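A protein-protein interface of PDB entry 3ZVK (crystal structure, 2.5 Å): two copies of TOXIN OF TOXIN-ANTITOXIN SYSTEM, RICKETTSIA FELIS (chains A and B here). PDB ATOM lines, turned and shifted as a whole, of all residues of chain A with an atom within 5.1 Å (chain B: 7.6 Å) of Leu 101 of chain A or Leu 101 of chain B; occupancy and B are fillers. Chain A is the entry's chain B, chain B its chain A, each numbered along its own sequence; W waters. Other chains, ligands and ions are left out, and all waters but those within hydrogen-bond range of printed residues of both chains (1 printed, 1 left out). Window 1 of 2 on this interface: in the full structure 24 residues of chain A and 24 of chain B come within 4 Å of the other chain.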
ATOM      1  N   ILE A  39     -32.062  24.394 -20.761  1.00  0.00           N
ATOM      2  CA  ILE A  39     -32.782  24.454 -19.477  1.00  0.00           C
ATOM      3  C   ILE A  39     -33.787  23.304 -19.407  1.00  0.00           C
ATOM      4  O   ILE A  39     -33.907  22.670 -18.361  1.00  0.00           O
ATOM      5  CB  ILE A  39     -33.428  25.840 -19.176  1.00  0.00           C
ATOM      6  CG1 ILE A  39     -32.406  27.014 -19.332  1.00  0.00           C
ATOM      7  CG2 ILE A  39     -34.112  25.847 -17.803  1.00  0.00           C
ATOM      8  CD1 ILE A  39     -31.029  26.909 -18.428  1.00  0.00           C
ATOM      9  N   ALA A  42     -31.824  20.138 -18.923  1.00  0.00           N
ATOM     10  CA  ALA A  42     -31.425  20.039 -17.517  1.00  0.00           C
ATOM     11  C   ALA A  42     -32.563  19.364 -16.723  1.00  0.00           C
ATOM     12  O   ALA A  42     -32.294  18.432 -15.961  1.00  0.00           O
ATOM     13  CB  ALA A  42     -31.131  21.417 -16.960  1.00  0.00           C
ATOM     14  N   PHE A  73     -28.348  28.222 -23.246  1.00  0.00           N
ATOM     15  CA  PHE A  73     -28.940  29.418 -22.636  1.00  0.00           C
ATOM     16  C   PHE A  73     -27.825  30.451 -22.649  1.00  0.00           C
ATOM     17  O   PHE A  73     -26.838  30.320 -21.940  1.00  0.00           O
ATOM     18  CB  PHE A  73     -29.491  29.123 -21.226  1.00  0.00           C
ATOM     19  CG  PHE A  73     -30.180  30.320 -20.620  1.00  0.00           C
ATOM     20  CD1 PHE A  73     -31.524  30.574 -20.879  1.00  0.00           C
ATOM     21  CD2 PHE A  73     -29.474  31.214 -19.812  1.00  0.00           C
ATOM     22  CE1 PHE A  73     -32.154  31.698 -20.336  1.00  0.00           C
ATOM     23  CE2 PHE A  73     -30.098  32.349 -19.288  1.00  0.00           C
ATOM     24  CZ  PHE A  73     -31.428  32.583 -19.554  1.00  0.00           C
ATOM     25  N   TYR A  81     -34.767  37.822 -19.679  1.00  0.00           N
ATOM     26  CA  TYR A  81     -35.107  37.165 -18.410  1.00  0.00           C
ATOM     27  C   TYR A  81     -35.287  38.229 -17.304  1.00  0.00           C
ATOM     28  O   TYR A  81     -36.236  38.151 -16.525  1.00  0.00           O
ATOM     29  CB  TYR A  81     -34.030  36.119 -18.027  1.00  0.00           C
ATOM     30  CG  TYR A  81     -34.149  35.606 -16.609  1.00  0.00           C
ATOM     31  CD1 TYR A  81     -33.496  36.250 -15.555  1.00  0.00           C
ATOM     32  CD2 TYR A  81     -34.878  34.464 -16.322  1.00  0.00           C
ATOM     33  CE1 TYR A  81     -33.596  35.784 -14.250  1.00  0.00           C
ATOM     34  CE2 TYR A  81     -34.970  33.977 -15.016  1.00  0.00           C
ATOM     35  CZ  TYR A  81     -34.326  34.639 -13.988  1.00  0.00           C
ATOM     36  OH  TYR A  81     -34.419  34.166 -12.708  1.00  0.00           O
ATOM     37  N   ASN A  97     -39.130  28.682 -11.361  1.00  0.00           N
ATOM     38  CA  ASN A  97     -37.775  29.075 -11.706  1.00  0.00           C
ATOM     39  C   ASN A  97     -37.296  28.731 -13.119  1.00  0.00           C
ATOM     40  O   ASN A  97     -36.719  29.578 -13.802  1.00  0.00           O
ATOM     41  CB  ASN A  97     -36.835  28.493 -10.688  1.00  0.00           C
ATOM     42  CG  ASN A  97     -35.612  29.291 -10.607  1.00  0.00           C
ATOM     43  OD1 ASN A  97     -35.636  30.420 -10.101  1.00  0.00           O
ATOM     44  ND2 ASN A  97     -34.545  28.738 -11.165  1.00  0.00           N
ATOM     45  N   ASN A  98     -37.516  27.475 -13.534  1.00  0.00           N
ATOM     46  CA  ASN A  98     -37.084  26.944 -14.815  1.00  0.00           C
ATOM     47  C   ASN A  98     -37.956  27.428 -15.939  1.00  0.00           C
ATOM     48  O   ASN A  98     -37.432  27.825 -16.965  1.00  0.00           O
ATOM     49  CB  ASN A  98     -37.000  25.419 -14.764  1.00  0.00           C
ATOM     50  CG  ASN A  98     -35.856  24.902 -13.916  1.00  0.00           C
ATOM     51  OD1 ASN A  98     -34.829  25.555 -13.744  1.00  0.00           O
ATOM     52  ND2 ASN A  98     -35.979  23.695 -13.419  1.00  0.00           N
ATOM     53  N   ASP A  99     -39.282  27.450 -15.740  1.00  0.00           N
ATOM     54  CA  ASP A  99     -40.261  27.930 -16.718  1.00  0.00           C
ATOM     55  C   ASP A  99     -39.987  29.368 -17.112  1.00  0.00           C
ATOM     56  O   ASP A  99     -40.142  29.726 -18.281  1.00  0.00           O
ATOM     57  CB  ASP A  99     -41.693  27.763 -16.171  1.00  0.00           C
ATOM     58  CG  ASP A  99     -42.192  26.329 -16.247  1.00  0.00           C
ATOM     59  OD1 ASP A  99     -41.632  25.547 -17.054  1.00  0.00           O
ATOM     60  OD2 ASP A  99     -43.134  25.981 -15.486  1.00  0.00           O
ATOM     61  N   LEU A 100     -39.532  30.172 -16.149  1.00  0.00           N
ATOM     62  CA  LEU A 100     -39.179  31.558 -16.334  1.00  0.00           C
ATOM     63  C   LEU A 100     -37.936  31.679 -17.236  1.00  0.00           C
ATOM     64  O   LEU A 100     -37.919  32.521 -18.129  1.00  0.00           O
ATOM     65  CB  LEU A 100     -38.963  32.171 -14.942  1.00  0.00           C
ATOM     66  CG  LEU A 100     -38.634  33.648 -14.828  1.00  0.00           C
ATOM     67  CD1 LEU A 100     -39.655  34.527 -15.547  1.00  0.00           C
ATOM     68  CD2 LEU A 100     -38.585  34.023 -13.376  1.00  0.00           C
ATOM     69  N   LEU A 101     -36.934  30.800 -17.055  1.00  0.00           N
ATOM     70  CA  LEU A 101     -35.730  30.732 -17.899  1.00  0.00           C
ATOM     71  C   LEU A 101     -36.085  30.227 -19.331  1.00  0.00           C
ATOM     72  O   LEU A 101     -35.593  30.786 -20.321  1.00  0.00           O
ATOM     73  CB  LEU A 101     -34.667  29.823 -17.269  1.00  0.00           C
ATOM     74  CG  LEU A 101     -33.892  30.367 -16.054  1.00  0.00           C
ATOM     75  CD1 LEU A 101     -33.258  29.236 -15.279  1.00  0.00           C
ATOM     76  CD2 LEU A 101     -32.794  31.334 -16.460  1.00  0.00           C
ATOM     77  N   ILE A 102     -36.950  29.177 -19.418  1.00  0.00           N
ATOM     78  CA  ILE A 102     -37.426  28.570 -20.671  1.00  0.00           C
ATOM     79  C   ILE A 102     -38.221  29.563 -21.535  1.00  0.00           C
ATOM     80  O   ILE A 102     -37.993  29.646 -22.749  1.00  0.00           O
ATOM     81  CB  ILE A 102     -38.177  27.230 -20.440  1.00  0.00           C
ATOM     82  CG1 ILE A 102     -37.238  26.185 -19.824  1.00  0.00           C
ATOM     83  CG2 ILE A 102     -38.728  26.688 -21.759  1.00  0.00           C
ATOM     84  CD1 ILE A 102     -37.938  25.139 -18.947  1.00  0.00           C
ATOM     85  N   ALA A 103     -39.123  30.320 -20.903  1.00  0.00           N
ATOM     86  CA  ALA A 103     -39.931  31.361 -21.539  1.00  0.00           C
ATOM     87  C   ALA A 103     -39.050  32.478 -22.107  1.00  0.00           C
ATOM     88  O   ALA A 103     -39.219  32.880 -23.257  1.00  0.00           O
ATOM     89  CB  ALA A 103     -40.898  31.951 -20.523  1.00  0.00           C
ATOM     90  N   SER A 104     -38.112  32.982 -21.293  1.00  0.00           N
ATOM     91  CA  SER A 104     -37.194  34.069 -21.660  1.00  0.00           C
ATOM     92  C   SER A 104     -36.253  33.671 -22.822  1.00  0.00           C
ATOM     93  O   SER A 104     -35.919  34.513 -23.647  1.00  0.00           O
ATOM     94  CB  SER A 104     -36.426  34.527 -20.429  1.00  0.00           C
ATOM     95  OG  SER A 104     -35.513  33.520 -20.028  1.00  0.00           O
ATOM     96  N   HIS A 105     -35.892  32.369 -22.903  1.00  0.00           N
ATOM     97  CA  HIS A 105     -35.080  31.791 -23.964  1.00  0.00           C
ATOM     98  C   HIS A 105     -35.878  31.784 -25.268  1.00  0.00           C
ATOM     99  O   HIS A 105     -35.334  32.131 -26.326  1.00  0.00           O
ATOM    100  CB  HIS A 105     -34.634  30.362 -23.603  1.00  0.00           C
ATOM    101  CG  HIS A 105     -33.437  29.881 -24.388  1.00  0.00           C
ATOM    102  ND1 HIS A 105     -32.824  28.671 -24.103  1.00  0.00           N
ATOM    103  CD2 HIS A 105     -32.783  30.464 -25.425  1.00  0.00           C
ATOM    104  CE1 HIS A 105     -31.813  28.572 -24.948  1.00  0.00           C
ATOM    105  NE2 HIS A 105     -31.740  29.633 -25.753  1.00  0.00           N
ATOM    106  N   SER B  37     -21.316  32.247 -15.317  1.00  0.00           N
ATOM    107  CA  SER B  37     -22.293  31.461 -16.045  1.00  0.00           C
ATOM    108  C   SER B  37     -23.304  32.456 -16.602  1.00  0.00           C
ATOM    109  O   SER B  37     -23.555  33.481 -15.981  1.00  0.00           O
ATOM    110  CB  SER B  37     -23.019  30.535 -15.066  1.00  0.00           C
ATOM    111  OG  SER B  37     -23.966  29.736 -15.751  1.00  0.00           O
ATOM    112  N   SER B  38     -23.911  32.149 -17.749  1.00  0.00           N
ATOM    113  CA  SER B  38     -24.998  32.962 -18.284  1.00  0.00           C
ATOM    114  C   SER B  38     -26.163  32.982 -17.244  1.00  0.00           C
ATOM    115  O   SER B  38     -26.901  33.970 -17.218  1.00  0.00           O
ATOM    116  CB  SER B  38     -25.462  32.441 -19.641  1.00  0.00           C
ATOM    117  OG  SER B  38     -25.814  31.066 -19.630  1.00  0.00           O
ATOM    118  N   ILE B  39     -26.264  31.929 -16.338  1.00  0.00           N
ATOM    119  CA  ILE B  39     -27.254  31.813 -15.232  1.00  0.00           C
ATOM    120  C   ILE B  39     -27.041  32.923 -14.170  1.00  0.00           C
ATOM    121  O   ILE B  39     -28.001  33.518 -13.699  1.00  0.00           O
ATOM    122  CB  ILE B  39     -27.336  30.375 -14.596  1.00  0.00           C
ATOM    123  CG1 ILE B  39     -27.443  29.234 -15.654  1.00  0.00           C
ATOM    124  CG2 ILE B  39     -28.459  30.290 -13.550  1.00  0.00           C
ATOM    125  CD1 ILE B  39     -28.657  29.324 -16.654  1.00  0.00           C
ATOM    126  N   VAL B  40     -25.793  33.225 -13.855  1.00  0.00           N
ATOM    127  CA  VAL B  40     -25.407  34.331 -12.967  1.00  0.00           C
ATOM    128  C   VAL B  40     -25.834  35.635 -13.620  1.00  0.00           C
ATOM    129  O   VAL B  40     -26.479  36.447 -12.964  1.00  0.00           O
ATOM    130  CB  VAL B  40     -23.891  34.357 -12.606  1.00  0.00           C
ATOM    131  CG1 VAL B  40     -23.511  35.661 -11.903  1.00  0.00           C
ATOM    132  CG2 VAL B  40     -23.517  33.147 -11.756  1.00  0.00           C
ATOM    133  N   ALA B  42     -28.179  36.135 -15.816  1.00  0.00           N
ATOM    134  CA  ALA B  42     -29.642  36.197 -15.783  1.00  0.00           C
ATOM    135  C   ALA B  42     -30.065  36.843 -14.464  1.00  0.00           C
ATOM    136  O   ALA B  42     -30.883  37.762 -14.466  1.00  0.00           O
ATOM    137  CB  ALA B  42     -30.229  34.807 -15.904  1.00  0.00           C
ATOM    138  N   GLU B  43     -29.461  36.406 -13.338  1.00  0.00           N
ATOM    139  CA  GLU B  43     -29.745  36.946 -12.010  1.00  0.00           C
ATOM    140  C   GLU B  43     -29.328  38.419 -11.887  1.00  0.00           C
ATOM    141  O   GLU B  43     -30.083  39.221 -11.350  1.00  0.00           O
ATOM    142  CB  GLU B  43     -29.073  36.098 -10.922  1.00  0.00           C
ATOM    143  CG  GLU B  43     -29.600  34.676 -10.795  1.00  0.00           C
ATOM    144  CD  GLU B  43     -30.974  34.482 -10.182  1.00  0.00           C
ATOM    145  OE1 GLU B  43     -31.371  35.282  -9.304  1.00  0.00           O
ATOM    146  OE2 GLU B  43     -31.669  33.534 -10.601  1.00  0.00           O
ATOM    147  N   PHE B  73     -24.828  28.371 -20.644  1.00  0.00           N
ATOM    148  CA  PHE B  73     -25.196  27.119 -19.981  1.00  0.00           C
ATOM    149  C   PHE B  73     -25.493  26.130 -21.116  1.00  0.00           C
ATOM    150  O   PHE B  73     -26.470  26.276 -21.846  1.00  0.00           O
ATOM    151  CB  PHE B  73     -26.380  27.307 -19.029  1.00  0.00           C
ATOM    152  CG  PHE B  73     -26.724  26.052 -18.273  1.00  0.00           C
ATOM    153  CD1 PHE B  73     -26.090  25.750 -17.080  1.00  0.00           C
ATOM    154  CD2 PHE B  73     -27.676  25.152 -18.771  1.00  0.00           C
ATOM    155  CE1 PHE B  73     -26.402  24.570 -16.378  1.00  0.00           C
ATOM    156  CE2 PHE B  73     -27.982  23.971 -18.081  1.00  0.00           C
ATOM    157  CZ  PHE B  73     -27.333  23.678 -16.891  1.00  0.00           C
ATOM    158  N   CYS B  77     -23.582  20.529 -19.313  1.00  0.00           N
ATOM    159  CA  CYS B  77     -23.914  20.801 -17.904  1.00  0.00           C
ATOM    160  C   CYS B  77     -25.122  20.047 -17.408  1.00  0.00           C
ATOM    161  O   CYS B  77     -25.230  19.801 -16.206  1.00  0.00           O
ATOM    162  CB  CYS B  77     -24.089  22.293 -17.660  1.00  0.00           C
ATOM    163  SG  CYS B  77     -22.808  23.323 -18.394  1.00  0.00           S
ATOM    164  N   THR B  78     -26.061  19.753 -18.323  1.00  0.00           N
ATOM    165  CA  THR B  78     -27.336  19.092 -18.044  1.00  0.00           C
ATOM    166  C   THR B  78     -27.228  17.748 -17.285  1.00  0.00           C
ATOM    167  O   THR B  78     -28.027  17.517 -16.362  1.00  0.00           O
ATOM    168  CB  THR B  78     -28.189  19.031 -19.311  1.00  0.00           C
ATOM    169  OG1 THR B  78     -27.626  18.084 -20.225  1.00  0.00           O
ATOM    170  CG2 THR B  78     -28.326  20.383 -19.982  1.00  0.00           C
ATOM    171  N   TYR B  81     -26.225  18.490 -13.622  1.00  0.00           N
ATOM    172  CA  TYR B  81     -27.401  19.067 -12.950  1.00  0.00           C
ATOM    173  C   TYR B  81     -28.362  17.965 -12.465  1.00  0.00           C
ATOM    174  O   TYR B  81     -28.809  18.011 -11.318  1.00  0.00           O
ATOM    175  CB  TYR B  81     -28.154  20.037 -13.901  1.00  0.00           C
ATOM    176  CG  TYR B  81     -29.473  20.524 -13.346  1.00  0.00           C
ATOM    177  CD1 TYR B  81     -29.531  21.640 -12.524  1.00  0.00           C
ATOM    178  CD2 TYR B  81     -30.664  19.869 -13.641  1.00  0.00           C
ATOM    179  CE1 TYR B  81     -30.744  22.108 -12.028  1.00  0.00           C
ATOM    180  CE2 TYR B  81     -31.881  20.309 -13.125  1.00  0.00           C
ATOM    181  CZ  TYR B  81     -31.917  21.442 -12.335  1.00  0.00           C
ATOM    182  OH  TYR B  81     -33.107  21.896 -11.831  1.00  0.00           O
ATOM    183  N   LEU B  84     -26.694  15.902  -9.577  1.00  0.00           N
ATOM    184  CA  LEU B  84     -26.561  16.744  -8.392  1.00  0.00           C
ATOM    185  C   LEU B  84     -27.917  16.998  -7.701  1.00  0.00           C
ATOM    186  O   LEU B  84     -28.027  16.817  -6.486  1.00  0.00           O
ATOM    187  CB  LEU B  84     -25.844  18.069  -8.759  1.00  0.00           C
ATOM    188  CG  LEU B  84     -25.632  19.107  -7.646  1.00  0.00           C
ATOM    189  CD1 LEU B  84     -24.831  18.529  -6.486  1.00  0.00           C
ATOM    190  CD2 LEU B  84     -24.951  20.353  -8.183  1.00  0.00           C
ATOM    191  N   ILE B  95     -30.291  23.376  -2.201  1.00  0.00           N
ATOM    192  CA  ILE B  95     -29.475  24.454  -2.773  1.00  0.00           C
ATOM    193  C   ILE B  95     -30.230  24.722  -4.063  1.00  0.00           C
ATOM    194  O   ILE B  95     -29.747  24.446  -5.169  1.00  0.00           O
ATOM    195  CB  ILE B  95     -27.960  24.107  -2.950  1.00  0.00           C
ATOM    196  CG1 ILE B  95     -27.250  23.907  -1.580  1.00  0.00           C
ATOM    197  CG2 ILE B  95     -27.217  25.165  -3.795  1.00  0.00           C
ATOM    198  CD1 ILE B  95     -27.289  25.133  -0.553  1.00  0.00           C
ATOM    199  N   GLY B  96     -31.468  25.169  -3.870  1.00  0.00           N
ATOM    200  CA  GLY B  96     -32.449  25.393  -4.910  1.00  0.00           C
ATOM    201  C   GLY B  96     -32.085  26.287  -6.073  1.00  0.00           C
ATOM    202  O   GLY B  96     -30.970  26.812  -6.182  1.00  0.00           O
ATOM    203  N   ASN B  97     -33.061  26.394  -6.980  1.00  0.00           N
ATOM    204  CA  ASN B  97     -33.124  27.234  -8.157  1.00  0.00           C
ATOM    205  C   ASN B  97     -31.916  27.243  -9.108  1.00  0.00           C
ATOM    206  O   ASN B  97     -31.454  26.207  -9.634  1.00  0.00           O
ATOM    207  CB  ASN B  97     -33.645  28.673  -7.765  1.00  0.00           C
ATOM    208  CG  ASN B  97     -32.657  29.761  -7.324  1.00  0.00           C
ATOM    209  OD1 ASN B  97     -31.578  29.514  -6.780  1.00  0.00           O
ATOM    210  ND2 ASN B  97     -33.005  31.012  -7.595  1.00  0.00           N
ATOM    211  N   ASN B  98     -31.445  28.460  -9.332  1.00  0.00           N
ATOM    212  CA  ASN B  98     -30.369  28.822 -10.174  1.00  0.00           C
ATOM    213  C   ASN B  98     -29.036  28.451  -9.575  1.00  0.00           C
ATOM    214  O   ASN B  98     -28.156  28.048 -10.338  1.00  0.00           O
ATOM    215  CB  ASN B  98     -30.568  30.268 -10.613  1.00  0.00           C
ATOM    216  CG  ASN B  98     -31.803  30.321 -11.481  1.00  0.00           C
ATOM    217  OD1 ASN B  98     -32.396  29.287 -11.747  1.00  0.00           O
ATOM    218  ND2 ASN B  98     -32.239  31.482 -11.953  1.00  0.00           N
ATOM    219  N   ASP B  99     -28.914  28.443  -8.235  1.00  0.00           N
ATOM    220  CA  ASP B  99     -27.672  28.010  -7.577  1.00  0.00           C
ATOM    221  C   ASP B  99     -27.300  26.557  -7.907  1.00  0.00           C
ATOM    222  O   ASP B  99     -26.132  26.270  -8.145  1.00  0.00           O
ATOM    223  CB  ASP B  99     -27.635  28.355  -6.084  1.00  0.00           C
ATOM    224  CG  ASP B  99     -27.414  29.842  -5.830  1.00  0.00           C
ATOM    225  OD1 ASP B  99     -27.127  30.579  -6.802  1.00  0.00           O
ATOM    226  OD2 ASP B  99     -27.493  30.266  -4.658  1.00  0.00           O
ATOM    227  N   LEU B 100     -28.314  25.684  -8.064  1.00  0.00           N
ATOM    228  CA  LEU B 100     -28.143  24.305  -8.528  1.00  0.00           C
ATOM    229  C   LEU B 100     -27.597  24.311 -10.013  1.00  0.00           C
ATOM    230  O   LEU B 100     -26.660  23.577 -10.322  1.00  0.00           O
ATOM    231  CB  LEU B 100     -29.495  23.582  -8.446  1.00  0.00           C
ATOM    232  CG  LEU B 100     -29.535  22.113  -8.019  1.00  0.00           C
ATOM    233  CD1 LEU B 100     -28.389  21.742  -7.125  1.00  0.00           C
ATOM    234  CD2 LEU B 100     -30.812  21.813  -7.257  1.00  0.00           C
ATOM    235  N   LEU B 101     -28.139  25.190 -10.883  1.00  0.00           N
ATOM    236  CA  LEU B 101     -27.710  25.334 -12.276  1.00  0.00           C
ATOM    237  C   LEU B 101     -26.284  25.883 -12.336  1.00  0.00           C
ATOM    238  O   LEU B 101     -25.458  25.379 -13.095  1.00  0.00           O
ATOM    239  CB  LEU B 101     -28.676  26.246 -13.078  1.00  0.00           C
ATOM    240  CG  LEU B 101     -30.047  25.643 -13.467  1.00  0.00           C
ATOM    241  CD1 LEU B 101     -31.012  26.704 -13.885  1.00  0.00           C
ATOM    242  CD2 LEU B 101     -29.921  24.695 -14.630  1.00  0.00           C
ATOM    243  N   ILE B 102     -26.010  26.913 -11.508  1.00  0.00           N
ATOM    244  CA  ILE B 102     -24.724  27.584 -11.369  1.00  0.00           C
ATOM    245  C   ILE B 102     -23.651  26.586 -10.948  1.00  0.00           C
ATOM    246  O   ILE B 102     -22.593  26.577 -11.572  1.00  0.00           O
ATOM    247  CB  ILE B 102     -24.844  28.828 -10.423  1.00  0.00           C
ATOM    248  CG1 ILE B 102     -25.620  29.958 -11.142  1.00  0.00           C
ATOM    249  CG2 ILE B 102     -23.462  29.345  -9.969  1.00  0.00           C
ATOM    250  CD1 ILE B 102     -26.526  30.824 -10.223  1.00  0.00           C
ATOM    251  N   ALA B 103     -23.932  25.744  -9.922  1.00  0.00           N
ATOM    252  CA  ALA B 103     -23.031  24.719  -9.370  1.00  0.00           C
ATOM    253  C   ALA B 103     -22.739  23.640 -10.403  1.00  0.00           C
ATOM    254  O   ALA B 103     -21.573  23.285 -10.594  1.00  0.00           O
ATOM    255  CB  ALA B 103     -23.627  24.111  -8.101  1.00  0.00           C
ATOM    256  N   SER B 104     -23.791  23.176 -11.113  1.00  0.00           N
ATOM    257  CA  SER B 104     -23.737  22.172 -12.196  1.00  0.00           C
ATOM    258  C   SER B 104     -22.778  22.620 -13.285  1.00  0.00           C
ATOM    259  O   SER B 104     -22.039  21.809 -13.828  1.00  0.00           O
ATOM    260  CB  SER B 104     -25.114  22.010 -12.839  1.00  0.00           C
ATOM    261  OG  SER B 104     -26.028  21.513 -11.881  1.00  0.00           O
ATOM    262  N   HIS B 105     -22.850  23.919 -13.626  1.00  0.00           N
ATOM    263  CA  HIS B 105     -22.064  24.600 -14.648  1.00  0.00           C
ATOM    264  C   HIS B 105     -20.586  24.603 -14.274  1.00  0.00           C
ATOM    265  O   HIS B 105     -19.777  24.244 -15.122  1.00  0.00           O
ATOM    266  CB  HIS B 105     -22.601  26.021 -14.917  1.00  0.00           C
ATOM    267  CG  HIS B 105     -22.205  26.565 -16.254  1.00  0.00           C
ATOM    268  ND1 HIS B 105     -22.683  27.772 -16.702  1.00  0.00           N
ATOM    269  CD2 HIS B 105     -21.375  26.057 -17.191  1.00  0.00           C
ATOM    270  CE1 HIS B 105     -22.153  27.954 -17.896  1.00  0.00           C
ATOM    271  NE2 HIS B 105     -21.375  26.940 -18.238  1.00  0.00           N
ATOM    272  N   ALA B 106     -20.234  24.951 -13.007  1.00  0.00           N
ATOM    273  CA  ALA B 106     -18.845  24.910 -12.533  1.00  0.00           C
ATOM    274  C   ALA B 106     -18.326  23.461 -12.581  1.00  0.00           C
ATOM    275  O   ALA B 106     -17.214  23.239 -13.057  1.00  0.00           O
ATOM    276  CB  ALA B 106     -18.738  25.476 -11.122  1.00  0.00           C
ATOM    277  N   ILE B 107     -19.149  22.475 -12.159  1.00  0.00           N
ATOM    278  CA  ILE B 107     -18.784  21.062 -12.187  1.00  0.00           C
ATOM    279  C   ILE B 107     -18.487  20.636 -13.628  1.00  0.00           C
ATOM    280  O   ILE B 107     -17.435  20.050 -13.885  1.00  0.00           O
ATOM    281  CB  ILE B 107     -19.841  20.150 -11.471  1.00  0.00           C
ATOM    282  CG1 ILE B 107     -19.899  20.397  -9.967  1.00  0.00           C
ATOM    283  CG2 ILE B 107     -19.550  18.657 -11.713  1.00  0.00           C
ATOM    284  CD1 ILE B 107     -21.195  19.960  -9.254  1.00  0.00           C
ATOM    285  N   ALA B 108     -19.391  20.962 -14.567  1.00  0.00           N
ATOM    286  CA  ALA B 108     -19.258  20.627 -15.988  1.00  0.00           C
ATOM    287  C   ALA B 108     -18.046  21.263 -16.673  1.00  0.00           C
ATOM    288  O   ALA B 108     -17.498  20.664 -17.606  1.00  0.00           O
ATOM    289  CB  ALA B 108     -20.515  20.993 -16.727  1.00  0.00           C
ATOM    290  N   PHE B 121     -23.648  27.602  -1.452  1.00  0.00           N
ATOM    291  CA  PHE B 121     -23.366  26.252  -1.962  1.00  0.00           C
ATOM    292  C   PHE B 121     -22.894  25.443  -0.787  1.00  0.00           C
ATOM    293  O   PHE B 121     -21.765  25.621  -0.312  1.00  0.00           O
ATOM    294  CB  PHE B 121     -22.337  26.269  -3.110  1.00  0.00           C
ATOM    295  CG  PHE B 121     -22.697  27.217  -4.212  1.00  0.00           C
ATOM    296  CD1 PHE B 121     -23.648  26.872  -5.161  1.00  0.00           C
ATOM    297  CD2 PHE B 121     -22.117  28.475  -4.282  1.00  0.00           C
ATOM    298  CE1 PHE B 121     -23.996  27.761  -6.184  1.00  0.00           C
ATOM    299  CE2 PHE B 121     -22.453  29.358  -5.311  1.00  0.00           C
ATOM    300  CZ  PHE B 121     -23.407  29.003  -6.246  1.00  0.00           C
HETATM  301  O   HOH W   1     -35.147  31.661 -12.615  1.00  0.00           O
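CD1 of Ile 39 of chain A touches CD2 of Phe 73 of chain B, at 3.8 Å. Thr 78 of chain B touches Ala 42 of chain A (CG2 to N, 3.7 Å). CD2 of Tyr 81 of chain B touches O of Ala 42 of chain A, 3.2 Å away. Ile 39 of chain B touches Phe 73 of chain A (CD1 to CD2, 3.8 Å). CD1 of Tyr 81 of chain A touches O of Ala 42 of chain B (3.2 Å). OH of Tyr 81 of chain A touches OE2 of Glu 43 of chain B, at 3.5 Å. Tyr 81 of chain A touches Asn 98 of chain B. Asn 97 of chain B touches Asn 97 of chain A. Tyr 81 of chain B touches Asn 98 of chain A. Asn 98 of chain A touches Leu 101 of chain B (OD1 to CD1, 3.99 Å).
OG of Ser 37 of chain B lies close to N of Ile 39 of chain B, at 3.2 Å. The backbone NH of Phe 73 of chain B is in hydrogen-bond range of the side-chain hydroxyl of Ser 38 of chain B (3.0 Å). The side-chain carboxylate (OE2) of Glu 43 of chain B is in hydrogen-bond range of the side-chain amide nitrogen (ND2) of Asn 98 of chain B (2.5 Å). N of Tyr 81 of chain B sits close to OG of Ser 104 of chain B (3.5 Å). The side-chain amide oxygen (OD1) of Asn 97 of chain B sits at hydrogen-bond distance from the backbone NH (N) of Asp 99 of chain B, 3.2 Å away. The side-chain hydroxyl (OG) of Ser 104 of chain A sits at hydrogen-bond distance from the backbone carbonyl oxygen (O) of Leu 101 of chain A (2.8 Å).
Of the 13 printed residues of chain A, 7 touch a printed residue of chain B. Hydrophobic or aromatic side chains of chain A within 4 Å of the printed part of chain B: Ile 39, Ala 42, Phe 73, Tyr 81 and Leu 101. Hydrophobic or aromatic side chains of chain B within 4 Å of the printed part of chain A: Ile 39, Ala 42, Phe 73, Tyr 81 and Leu 101.
Of chain B, only Asn 98 (3.6 Å) and Leu 101 (3.7 Å) come within 4 Å of Leu 101 of chain A. Printed residues of chain A within 4 Å of Ile 39 of chain B: Ile 39 (3.8 Å) and Phe 73 (3.8 Å). Printed residues of chain A within 4 Å of Glu 43 of chain B: Tyr 81. Of the printed residues of chain A, Ser 38 of chain B touches Phe 73. Val 40 of chain B touches none of the printed residues of chain A. Cys 77 of chain B touches none of the printed residues of chain A. The nearest printed residue of chain A that does not touch Leu 101 of chain B is Ala 42 of chain A (4.2 Å). The nearest printed residue of chain B that does not touch Asn 98 of chain A is Asn 98 of chain B (4.9 Å).
Ala 42 of chain A touches Tyr 81 of chain B, and with the chains exchanged Tyr 81 of chain A touches Ala 42 of chain B. Tyr 81 of chain A touches Asn 98 of chain B, and with the chains exchanged Asn 98 of chain A touches Tyr 81 of chain B. Asn 97 of chain A touches its own counterpart, Asn 97 of chain B. Asn 98 of chain A touches Leu 101 of chain B, and with the chains exchanged Leu 101 of chain A touches Asn 98 of chain B. Positions printed for both chains: 39, 42, 73, 81, 97, 98, 99, 100, 101, 102, 103, 104 and 105.
The backbone carbonyl oxygen (O) of Phe 73 of chain A is in hydrogen-bond range of the side-chain hydroxyl (OG) of Ser 38 of chain B (2.6 Å). The backbone carbonyl oxygen (O) of Phe 73 of chain B is in hydrogen-bond range of the backbone NH (N) of Phe 73 of chain A. The side-chain amide oxygen (OD1) of Asn 98 of chain B lies close to the side-chain amide nitrogen (ND2) of Asn 97 of chain A (2.3 Å).
Water W1 lies within hydrogen-bond range of the side-chain hydroxyl (OH) of Tyr 81 of chain A (2.6 Å), the side-chain amide oxygen (OD1) of Asn 97 of chain A (2.8 Å) and the side-chain amide nitrogen (ND2) of Asn 98 of chain B (3.0 Å).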
